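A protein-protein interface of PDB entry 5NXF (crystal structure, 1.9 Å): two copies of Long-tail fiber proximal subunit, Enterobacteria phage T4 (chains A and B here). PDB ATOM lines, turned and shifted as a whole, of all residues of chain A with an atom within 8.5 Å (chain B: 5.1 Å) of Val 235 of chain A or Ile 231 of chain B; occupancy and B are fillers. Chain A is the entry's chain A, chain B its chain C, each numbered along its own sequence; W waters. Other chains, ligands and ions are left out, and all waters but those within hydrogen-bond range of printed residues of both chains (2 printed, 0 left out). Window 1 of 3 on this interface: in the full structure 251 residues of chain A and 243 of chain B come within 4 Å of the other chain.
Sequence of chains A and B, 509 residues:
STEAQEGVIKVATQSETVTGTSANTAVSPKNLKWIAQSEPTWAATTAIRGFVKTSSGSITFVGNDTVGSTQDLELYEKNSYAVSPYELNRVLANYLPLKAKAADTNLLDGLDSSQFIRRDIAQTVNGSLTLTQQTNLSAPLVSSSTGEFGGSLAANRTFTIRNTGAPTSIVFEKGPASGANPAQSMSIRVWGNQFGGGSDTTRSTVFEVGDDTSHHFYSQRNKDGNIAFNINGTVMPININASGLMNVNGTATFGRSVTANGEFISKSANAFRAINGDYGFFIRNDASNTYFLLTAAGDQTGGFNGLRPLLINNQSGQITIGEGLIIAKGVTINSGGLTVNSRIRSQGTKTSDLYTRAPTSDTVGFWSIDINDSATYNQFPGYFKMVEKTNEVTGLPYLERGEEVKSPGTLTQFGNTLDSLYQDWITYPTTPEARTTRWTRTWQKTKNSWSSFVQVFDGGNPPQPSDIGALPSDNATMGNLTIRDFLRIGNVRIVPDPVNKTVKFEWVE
Phe 229 of chain A touches its own counterpart, Phe 229 of chain B. Ile 231 of chain A touches Phe 229 of chain B, but with the chains exchanged Phe 229 of chain A does not touch Ile 231 of chain B (6.4 Å). Thr 234 of chain A touches Phe 229 of chain B, but with the chains exchanged Phe 229 of chain A does not touch Thr 234 of chain B (11.0 Å). Val 235 of chain A touches Ile 231 of chain B, but with the chains exchanged Ile 231 of chain A does not touch Val 235 of chain B (6.8 Å). Positions printed for both chains: 229, 230, 231, 232, 233, 234 and 235. Of the 17 pairs that touch across the chains among the printed residues, 1 has its exchanged pair printed and touching as well.
Asn 230 of chain A touches none of the printed residues of chain B. Printed residues of chain B within 4 Å of Val 235 of chain A: Phe 229 and Ile 231. Printed residues of chain B within 4 Å of Ile 238 of chain A: Ile 231 (3.7 Å) and Gly 233 (3.0 Å). Printed residues of chain A within 4 Å of Phe 229 of chain B: Phe 229 (3.6 Å), Ile 231 (3.6 Å), Thr 234 (2.7 Å), Val 235 (3.4 Å) and Met 236 (2.8 Å). Of the printed residues of chain A, Ile 231 of chain B touches Val 235 (3.98 Å), Met 236 (3.0 Å), Pro 237 (3.5 Å) and Ile 238 (3.7 Å). Asn 232 of chain B touches none of the printed residues of chain A. Gly 233 of chain B touches just these residues of chain A: Pro 237, Ile 238 and Asn 239. Printed residues of chain A within 4 Å of Val 235 of chain B: Pro 237 (3.7 Å), Asn 239 (3.0 Å) and Ile 240 (3.5 Å). The nearest printed residue of chain A that does not touch Ile 231 of chain B is Ile 231 of chain A (5.7 Å). The nearest printed residue of chain B that does not touch Ile 240 of chain A is Thr 234 of chain B (4.4 Å).
The backbone carbonyl oxygen of Asn 239 of chain A is in hydrogen-bond range of the backbone NH of Val 235 of chain B (3.0 Å). O of Met 236 of chain A sits at hydrogen-bond distance from N of Ile 231 of chain B (3.0 Å). O of Gly 233 of chain B lies within hydrogen-bond range of N of Ile 238 of chain A (3.0 Å). The backbone NH of Met 236 of chain A is in hydrogen-bond range of the backbone carbonyl oxygen of Phe 229 of chain B. O of Thr 234 of chain A is in hydrogen-bond range of N of Phe 229 of chain B (2.7 Å).
Phe 229 of chain A touches Phe 229 of chain B. CA of Val 235 of chain A touches O of Phe 229 of chain B (3.4 Å). Asn 230 of chain B touches Met 236 of chain A. O of Ile 231 of chain B touches CA of Pro 237 of chain A (3.5 Å). Gly 233 of chain B touches Pro 237 of chain A. Pro 237 of chain A touches Val 235 of chain B. Ile 238 of chain A touches Ile 231 of chain B. Gly 233 of chain B touches Asn 239 of chain A. Thr 234 of chain B touches Asn 239 of chain A. Ile 240 of chain A touches Val 235 of chain B (CA to O, 3.5 Å).
Water W2 lies within hydrogen-bond range of the side-chain hydroxyl of Thr 234 of chain B (2.6 Å) and the backbone NH of Asn 239 of chain A (3.1 Å). Water W1 lies within hydrogen-bond range of O of Ile 231 of chain B (2.9 Å), O of Met 236 of chain A (3.1 Å) and ND2 of Asn 230 of chain B (3.4 Å).
Hydrophobic or aromatic side chains of chain A that line the printed part of chain B: Phe 229, Ile 231, Val 235, Met 236, Pro 237, Ile 238 and Ile 240. Printed residues of chain B that touch a printed residue of chain A: Phe 229, Asn 230, Ile 231, Gly 233, Thr 234 and Val 235. Hydrophobic or aromatic side chains of chain B that line the printed part of chain A: Phe 229, Ile 231 and Val 235. Among the printed residues, 17 pairs touch across the chains.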
ATOM      1  N   PHE A 229       3.585 -18.975  -6.872  1.00  0.00           N
ATOM      2  CA  PHE A 229       3.031 -18.289  -5.706  1.00  0.00           C
ATOM      3  C   PHE A 229       4.134 -17.336  -5.190  1.00  0.00           C
ATOM      4  O   PHE A 229       5.124 -17.762  -4.544  1.00  0.00           O
ATOM      5  CB  PHE A 229       2.604 -19.309  -4.641  1.00  0.00           C
ATOM      6  CG  PHE A 229       1.778 -18.709  -3.532  1.00  0.00           C
ATOM      7  CD1 PHE A 229       2.388 -18.023  -2.471  1.00  0.00           C
ATOM      8  CD2 PHE A 229       0.400 -18.771  -3.571  1.00  0.00           C
ATOM      9  CE1 PHE A 229       1.613 -17.440  -1.449  1.00  0.00           C
ATOM     10  CE2 PHE A 229      -0.378 -18.191  -2.566  1.00  0.00           C
ATOM     11  CZ  PHE A 229       0.237 -17.534  -1.499  1.00  0.00           C
ATOM     12  N   ASN A 230       4.005 -16.065  -5.538  1.00  0.00           N
ATOM     13  CA  ASN A 230       5.030 -15.068  -5.264  1.00  0.00           C
ATOM     14  C   ASN A 230       4.713 -14.393  -3.939  1.00  0.00           C
ATOM     15  O   ASN A 230       3.595 -13.916  -3.740  1.00  0.00           O
ATOM     16  CB  ASN A 230       5.072 -14.012  -6.364  1.00  0.00           C
ATOM     17  CG  ASN A 230       6.198 -13.000  -6.166  1.00  0.00           C
ATOM     18  OD1 ASN A 230       6.018 -11.982  -5.503  1.00  0.00           O
ATOM     19  ND2 ASN A 230       7.378 -13.304  -6.689  1.00  0.00           N
ATOM     20  N   ILE A 231       5.686 -14.355  -3.049  1.00  0.00           N
ATOM     21  CA  ILE A 231       5.543 -13.658  -1.779  1.00  0.00           C
ATOM     22  C   ILE A 231       6.548 -12.504  -1.801  1.00  0.00           C
ATOM     23  O   ILE A 231       7.770 -12.715  -1.939  1.00  0.00           O
ATOM     24  CB  ILE A 231       5.780 -14.607  -0.609  1.00  0.00           C
ATOM     25  CG1 ILE A 231       4.666 -15.657  -0.562  1.00  0.00           C
ATOM     26  CG2 ILE A 231       5.864 -13.856   0.720  1.00  0.00           C
ATOM     27  CD1 ILE A 231       5.025 -16.845   0.274  1.00  0.00           C
ATOM     28  N   ASN A 232       6.029 -11.291  -1.629  1.00  0.00           N
ATOM     29  CA  ASN A 232       6.829 -10.069  -1.722  1.00  0.00           C
ATOM     30  C   ASN A 232       7.509  -9.745  -0.364  1.00  0.00           C
ATOM     31  O   ASN A 232       7.418  -8.636   0.154  1.00  0.00           O
ATOM     32  CB  ASN A 232       5.941  -8.927  -2.208  1.00  0.00           C
ATOM     33  CG  ASN A 232       6.733  -7.727  -2.635  1.00  0.00           C
ATOM     34  OD1 ASN A 232       7.903  -7.857  -2.933  1.00  0.00           O
ATOM     35  ND2 ASN A 232       6.106  -6.560  -2.656  1.00  0.00           N
ATOM     36  N   GLY A 233       8.244 -10.723   0.164  1.00  0.00           N
ATOM     37  CA  GLY A 233       8.829 -10.635   1.489  1.00  0.00           C
ATOM     38  C   GLY A 233       9.188 -12.011   2.006  1.00  0.00           C
ATOM     39  O   GLY A 233       9.585 -12.880   1.217  1.00  0.00           O
ATOM     40  N   THR A 234       9.032 -12.216   3.314  1.00  0.00           N
ATOM     41  CA  THR A 234       9.475 -13.422   3.981  1.00  0.00           C
ATOM     42  C   THR A 234       8.339 -14.384   4.209  1.00  0.00           C
ATOM     43  O   THR A 234       7.307 -13.992   4.775  1.00  0.00           O
ATOM     44  CB  THR A 234      10.092 -13.059   5.347  1.00  0.00           C
ATOM     45  OG1 THR A 234      11.122 -12.103   5.130  1.00  0.00           O
ATOM     46  CG2 THR A 234      10.679 -14.260   6.053  1.00  0.00           C
ATOM     47  N   VAL A 235       8.520 -15.624   3.764  1.00  0.00           N
ATOM     48  CA  VAL A 235       7.604 -16.719   4.064  1.00  0.00           C
ATOM     49  C   VAL A 235       8.022 -17.397   5.359  1.00  0.00           C
ATOM     50  O   VAL A 235       9.198 -17.721   5.554  1.00  0.00           O
ATOM     51  CB  VAL A 235       7.443 -17.744   2.903  1.00  0.00           C
ATOM     52  CG1 VAL A 235       8.718 -18.563   2.647  1.00  0.00           C
ATOM     53  CG2 VAL A 235       6.262 -18.662   3.178  1.00  0.00           C
ATOM     54  N   MET A 236       7.054 -17.559   6.255  1.00  0.00           N
ATOM     55  CA  MET A 236       7.318 -17.990   7.601  1.00  0.00           C
ATOM     56  C   MET A 236       6.407 -19.137   7.941  1.00  0.00           C
ATOM     57  O   MET A 236       5.390 -18.938   8.636  1.00  0.00           O
ATOM     58  CB  MET A 236       7.158 -16.838   8.595  1.00  0.00           C
ATOM     59  CG  MET A 236       8.156 -15.754   8.262  1.00  0.00           C
ATOM     60  SD  MET A 236       8.049 -14.302   9.576  1.00  0.00           S
ATOM     61  CE  MET A 236       9.143 -15.179  10.972  1.00  0.00           C
ATOM     62  N   PRO A 237       6.755 -20.349   7.464  1.00  0.00           N
ATOM     63  CA  PRO A 237       6.030 -21.549   7.863  1.00  0.00           C
ATOM     64  C   PRO A 237       6.618 -22.187   9.122  1.00  0.00           C
ATOM     65  O   PRO A 237       7.639 -21.716   9.637  1.00  0.00           O
ATOM     66  CB  PRO A 237       6.251 -22.479   6.662  1.00  0.00           C
ATOM     67  CG  PRO A 237       7.664 -22.189   6.296  1.00  0.00           C
ATOM     68  CD  PRO A 237       7.847 -20.695   6.522  1.00  0.00           C
ATOM     69  N   ILE A 238       5.979 -23.252   9.587  1.00  0.00           N
ATOM     70  CA  ILE A 238       6.549 -24.134  10.585  1.00  0.00           C
ATOM     71  C   ILE A 238       7.439 -25.113   9.789  1.00  0.00           C
ATOM     72  O   ILE A 238       8.645 -24.826   9.621  1.00  0.00           O
ATOM     73  CB  ILE A 238       5.484 -24.802  11.480  1.00  0.00           C
ATOM     74  CG1 ILE A 238       4.680 -23.718  12.239  1.00  0.00           C
ATOM     75  CG2 ILE A 238       6.134 -25.789  12.457  1.00  0.00           C
ATOM     76  CD1 ILE A 238       3.624 -24.276  13.190  1.00  0.00           C
ATOM     77  N   ASN A 239       6.861 -26.175   9.241  1.00  0.00           N
ATOM     78  CA  ASN A 239       7.605 -27.109   8.396  1.00  0.00           C
ATOM     79  C   ASN A 239       7.528 -26.726   6.909  1.00  0.00           C
ATOM     80  O   ASN A 239       6.638 -25.994   6.478  1.00  0.00           O
ATOM     81  CB  ASN A 239       7.102 -28.540   8.565  1.00  0.00           C
ATOM     82  CG  ASN A 239       7.350 -29.106   9.959  1.00  0.00           C
ATOM     83  OD1 ASN A 239       8.092 -28.548  10.780  1.00  0.00           O
ATOM     84  ND2 ASN A 239       6.744 -30.240  10.214  1.00  0.00           N
ATOM     85  N   ILE A 240       8.478 -27.243   6.134  1.00  0.00           N
ATOM     86  CA  ILE A 240       8.504 -27.088   4.667  1.00  0.00           C
ATOM     87  C   ILE A 240       8.597 -28.494   4.135  1.00  0.00           C
ATOM     88  O   ILE A 240       9.422 -29.283   4.618  1.00  0.00           O
ATOM     89  CB  ILE A 240       9.724 -26.295   4.168  1.00  0.00           C
ATOM     90  CG1 ILE A 240       9.607 -24.830   4.553  1.00  0.00           C
ATOM     91  CG2 ILE A 240       9.921 -26.454   2.636  1.00  0.00           C
ATOM     92  CD1 ILE A 240      10.919 -24.056   4.455  1.00  0.00           C
ATOM     93  N   HIS B 216      -5.086 -19.965   9.528  1.00  0.00           N
ATOM     94  CA  HIS B 216      -4.335 -20.876   8.664  1.00  0.00           C
ATOM     95  C   HIS B 216      -3.104 -20.170   8.167  1.00  0.00           C
ATOM     96  O   HIS B 216      -1.993 -20.745   8.210  1.00  0.00           O
ATOM     97  CB  HIS B 216      -5.168 -21.314   7.471  1.00  0.00           C
ATOM     98  CG  HIS B 216      -6.292 -22.233   7.813  1.00  0.00           C
ATOM     99  ND1 HIS B 216      -6.846 -23.102   6.895  1.00  0.00           N
ATOM    100  CD2 HIS B 216      -6.975 -22.420   8.967  1.00  0.00           C
ATOM    101  CE1 HIS B 216      -7.832 -23.764   7.463  1.00  0.00           C
ATOM    102  NE2 HIS B 216      -7.919 -23.384   8.726  1.00  0.00           N
ATOM    103  N   PHE B 217      -3.303 -18.938   7.674  1.00  0.00           N
ATOM    104  CA  PHE B 217      -2.217 -18.112   7.196  1.00  0.00           C
ATOM    105  C   PHE B 217      -2.573 -16.637   7.212  1.00  0.00           C
ATOM    106  O   PHE B 217      -3.746 -16.280   7.295  1.00  0.00           O
ATOM    107  CB  PHE B 217      -1.803 -18.552   5.762  1.00  0.00           C
ATOM    108  CG  PHE B 217      -2.860 -18.315   4.697  1.00  0.00           C
ATOM    109  CD1 PHE B 217      -3.849 -19.256   4.449  1.00  0.00           C
ATOM    110  CD2 PHE B 217      -2.857 -17.146   3.923  1.00  0.00           C
ATOM    111  CE1 PHE B 217      -4.833 -19.043   3.471  1.00  0.00           C
ATOM    112  CE2 PHE B 217      -3.826 -16.936   2.932  1.00  0.00           C
ATOM    113  CZ  PHE B 217      -4.810 -17.895   2.704  1.00  0.00           C
ATOM    114  N   PHE B 229       4.667 -13.509   5.108  1.00  0.00           N
ATOM    115  CA  PHE B 229       3.579 -14.430   4.804  1.00  0.00           C
ATOM    116  C   PHE B 229       3.710 -15.601   5.758  1.00  0.00           C
ATOM    117  O   PHE B 229       4.599 -16.483   5.597  1.00  0.00           O
ATOM    118  CB  PHE B 229       3.598 -14.876   3.332  1.00  0.00           C
ATOM    119  CG  PHE B 229       2.352 -15.627   2.897  1.00  0.00           C
ATOM    120  CD1 PHE B 229       2.170 -16.972   3.202  1.00  0.00           C
ATOM    121  CD2 PHE B 229       1.367 -14.980   2.164  1.00  0.00           C
ATOM    122  CE1 PHE B 229       1.014 -17.658   2.789  1.00  0.00           C
ATOM    123  CE2 PHE B 229       0.211 -15.641   1.775  1.00  0.00           C
ATOM    124  CZ  PHE B 229       0.026 -16.985   2.083  1.00  0.00           C
ATOM    125  N   ASN B 230       2.867 -15.588   6.782  1.00  0.00           N
ATOM    126  CA  ASN B 230       2.925 -16.578   7.863  1.00  0.00           C
ATOM    127  C   ASN B 230       1.999 -17.740   7.569  1.00  0.00           C
ATOM    128  O   ASN B 230       0.838 -17.531   7.224  1.00  0.00           O
ATOM    129  CB  ASN B 230       2.513 -15.945   9.198  1.00  0.00           C
ATOM    130  CG  ASN B 230       2.746 -16.878  10.381  1.00  0.00           C
ATOM    131  OD1 ASN B 230       1.915 -17.734  10.689  1.00  0.00           O
ATOM    132  ND2 ASN B 230       3.898 -16.735  11.024  1.00  0.00           N
ATOM    133  N   ILE B 231       2.509 -18.959   7.718  1.00  0.00           N
ATOM    134  CA  ILE B 231       1.740 -20.191   7.501  1.00  0.00           C
ATOM    135  C   ILE B 231       1.788 -20.966   8.800  1.00  0.00           C
ATOM    136  O   ILE B 231       2.864 -21.320   9.269  1.00  0.00           O
ATOM    137  CB  ILE B 231       2.335 -21.049   6.342  1.00  0.00           C
ATOM    138  CG1 ILE B 231       2.115 -20.314   5.002  1.00  0.00           C
ATOM    139  CG2 ILE B 231       1.751 -22.479   6.338  1.00  0.00           C
ATOM    140  CD1 ILE B 231       2.969 -20.804   3.835  1.00  0.00           C
ATOM    141  N   ASN B 232       0.618 -21.259   9.361  1.00  0.00           N
ATOM    142  CA  ASN B 232       0.506 -21.836  10.704  1.00  0.00           C
ATOM    143  C   ASN B 232       0.559 -23.343  10.616  1.00  0.00           C
ATOM    144  O   ASN B 232      -0.317 -24.052  11.107  1.00  0.00           O
ATOM    145  CB  ASN B 232      -0.799 -21.374  11.352  1.00  0.00           C
ATOM    146  CG  ASN B 232      -0.832 -21.595  12.850  1.00  0.00           C
ATOM    147  OD1 ASN B 232       0.204 -21.800  13.475  1.00  0.00           O
ATOM    148  ND2 ASN B 232      -2.042 -21.515  13.441  1.00  0.00           N
ATOM    149  N   GLY B 233       1.631 -23.838  10.009  1.00  0.00           N
ATOM    150  CA  GLY B 233       1.745 -25.239   9.695  1.00  0.00           C
ATOM    151  C   GLY B 233       2.735 -25.479   8.578  1.00  0.00           C
ATOM    152  O   GLY B 233       3.691 -24.738   8.431  1.00  0.00           O
ATOM    153  N   THR B 234       2.489 -26.526   7.806  1.00  0.00           N
ATOM    154  CA  THR B 234       3.442 -27.003   6.812  1.00  0.00           C
ATOM    155  C   THR B 234       3.157 -26.372   5.440  1.00  0.00           C
ATOM    156  O   THR B 234       2.030 -26.413   4.938  1.00  0.00           O
ATOM    157  CB  THR B 234       3.392 -28.514   6.726  1.00  0.00           C
ATOM    158  OG1 THR B 234       3.624 -29.052   8.036  1.00  0.00           O
ATOM    159  CG2 THR B 234       4.467 -29.064   5.735  1.00  0.00           C
ATOM    160  N   VAL B 235       4.171 -25.783   4.841  1.00  0.00           N
ATOM    161  CA  VAL B 235       4.050 -25.301   3.463  1.00  0.00           C
ATOM    162  C   VAL B 235       4.515 -26.429   2.518  1.00  0.00           C
ATOM    163  O   VAL B 235       5.573 -27.026   2.721  1.00  0.00           O
ATOM    164  CB  VAL B 235       4.775 -23.952   3.211  1.00  0.00           C
ATOM    165  CG1 VAL B 235       6.298 -24.054   3.349  1.00  0.00           C
ATOM    166  CG2 VAL B 235       4.416 -23.429   1.831  1.00  0.00           C
HETATM  167  O   HOH W   1       4.425 -20.093  11.393  1.00  0.00           O
HETATM  168  O   HOH W   2       4.366 -27.762  10.171  1.00  0.00           O
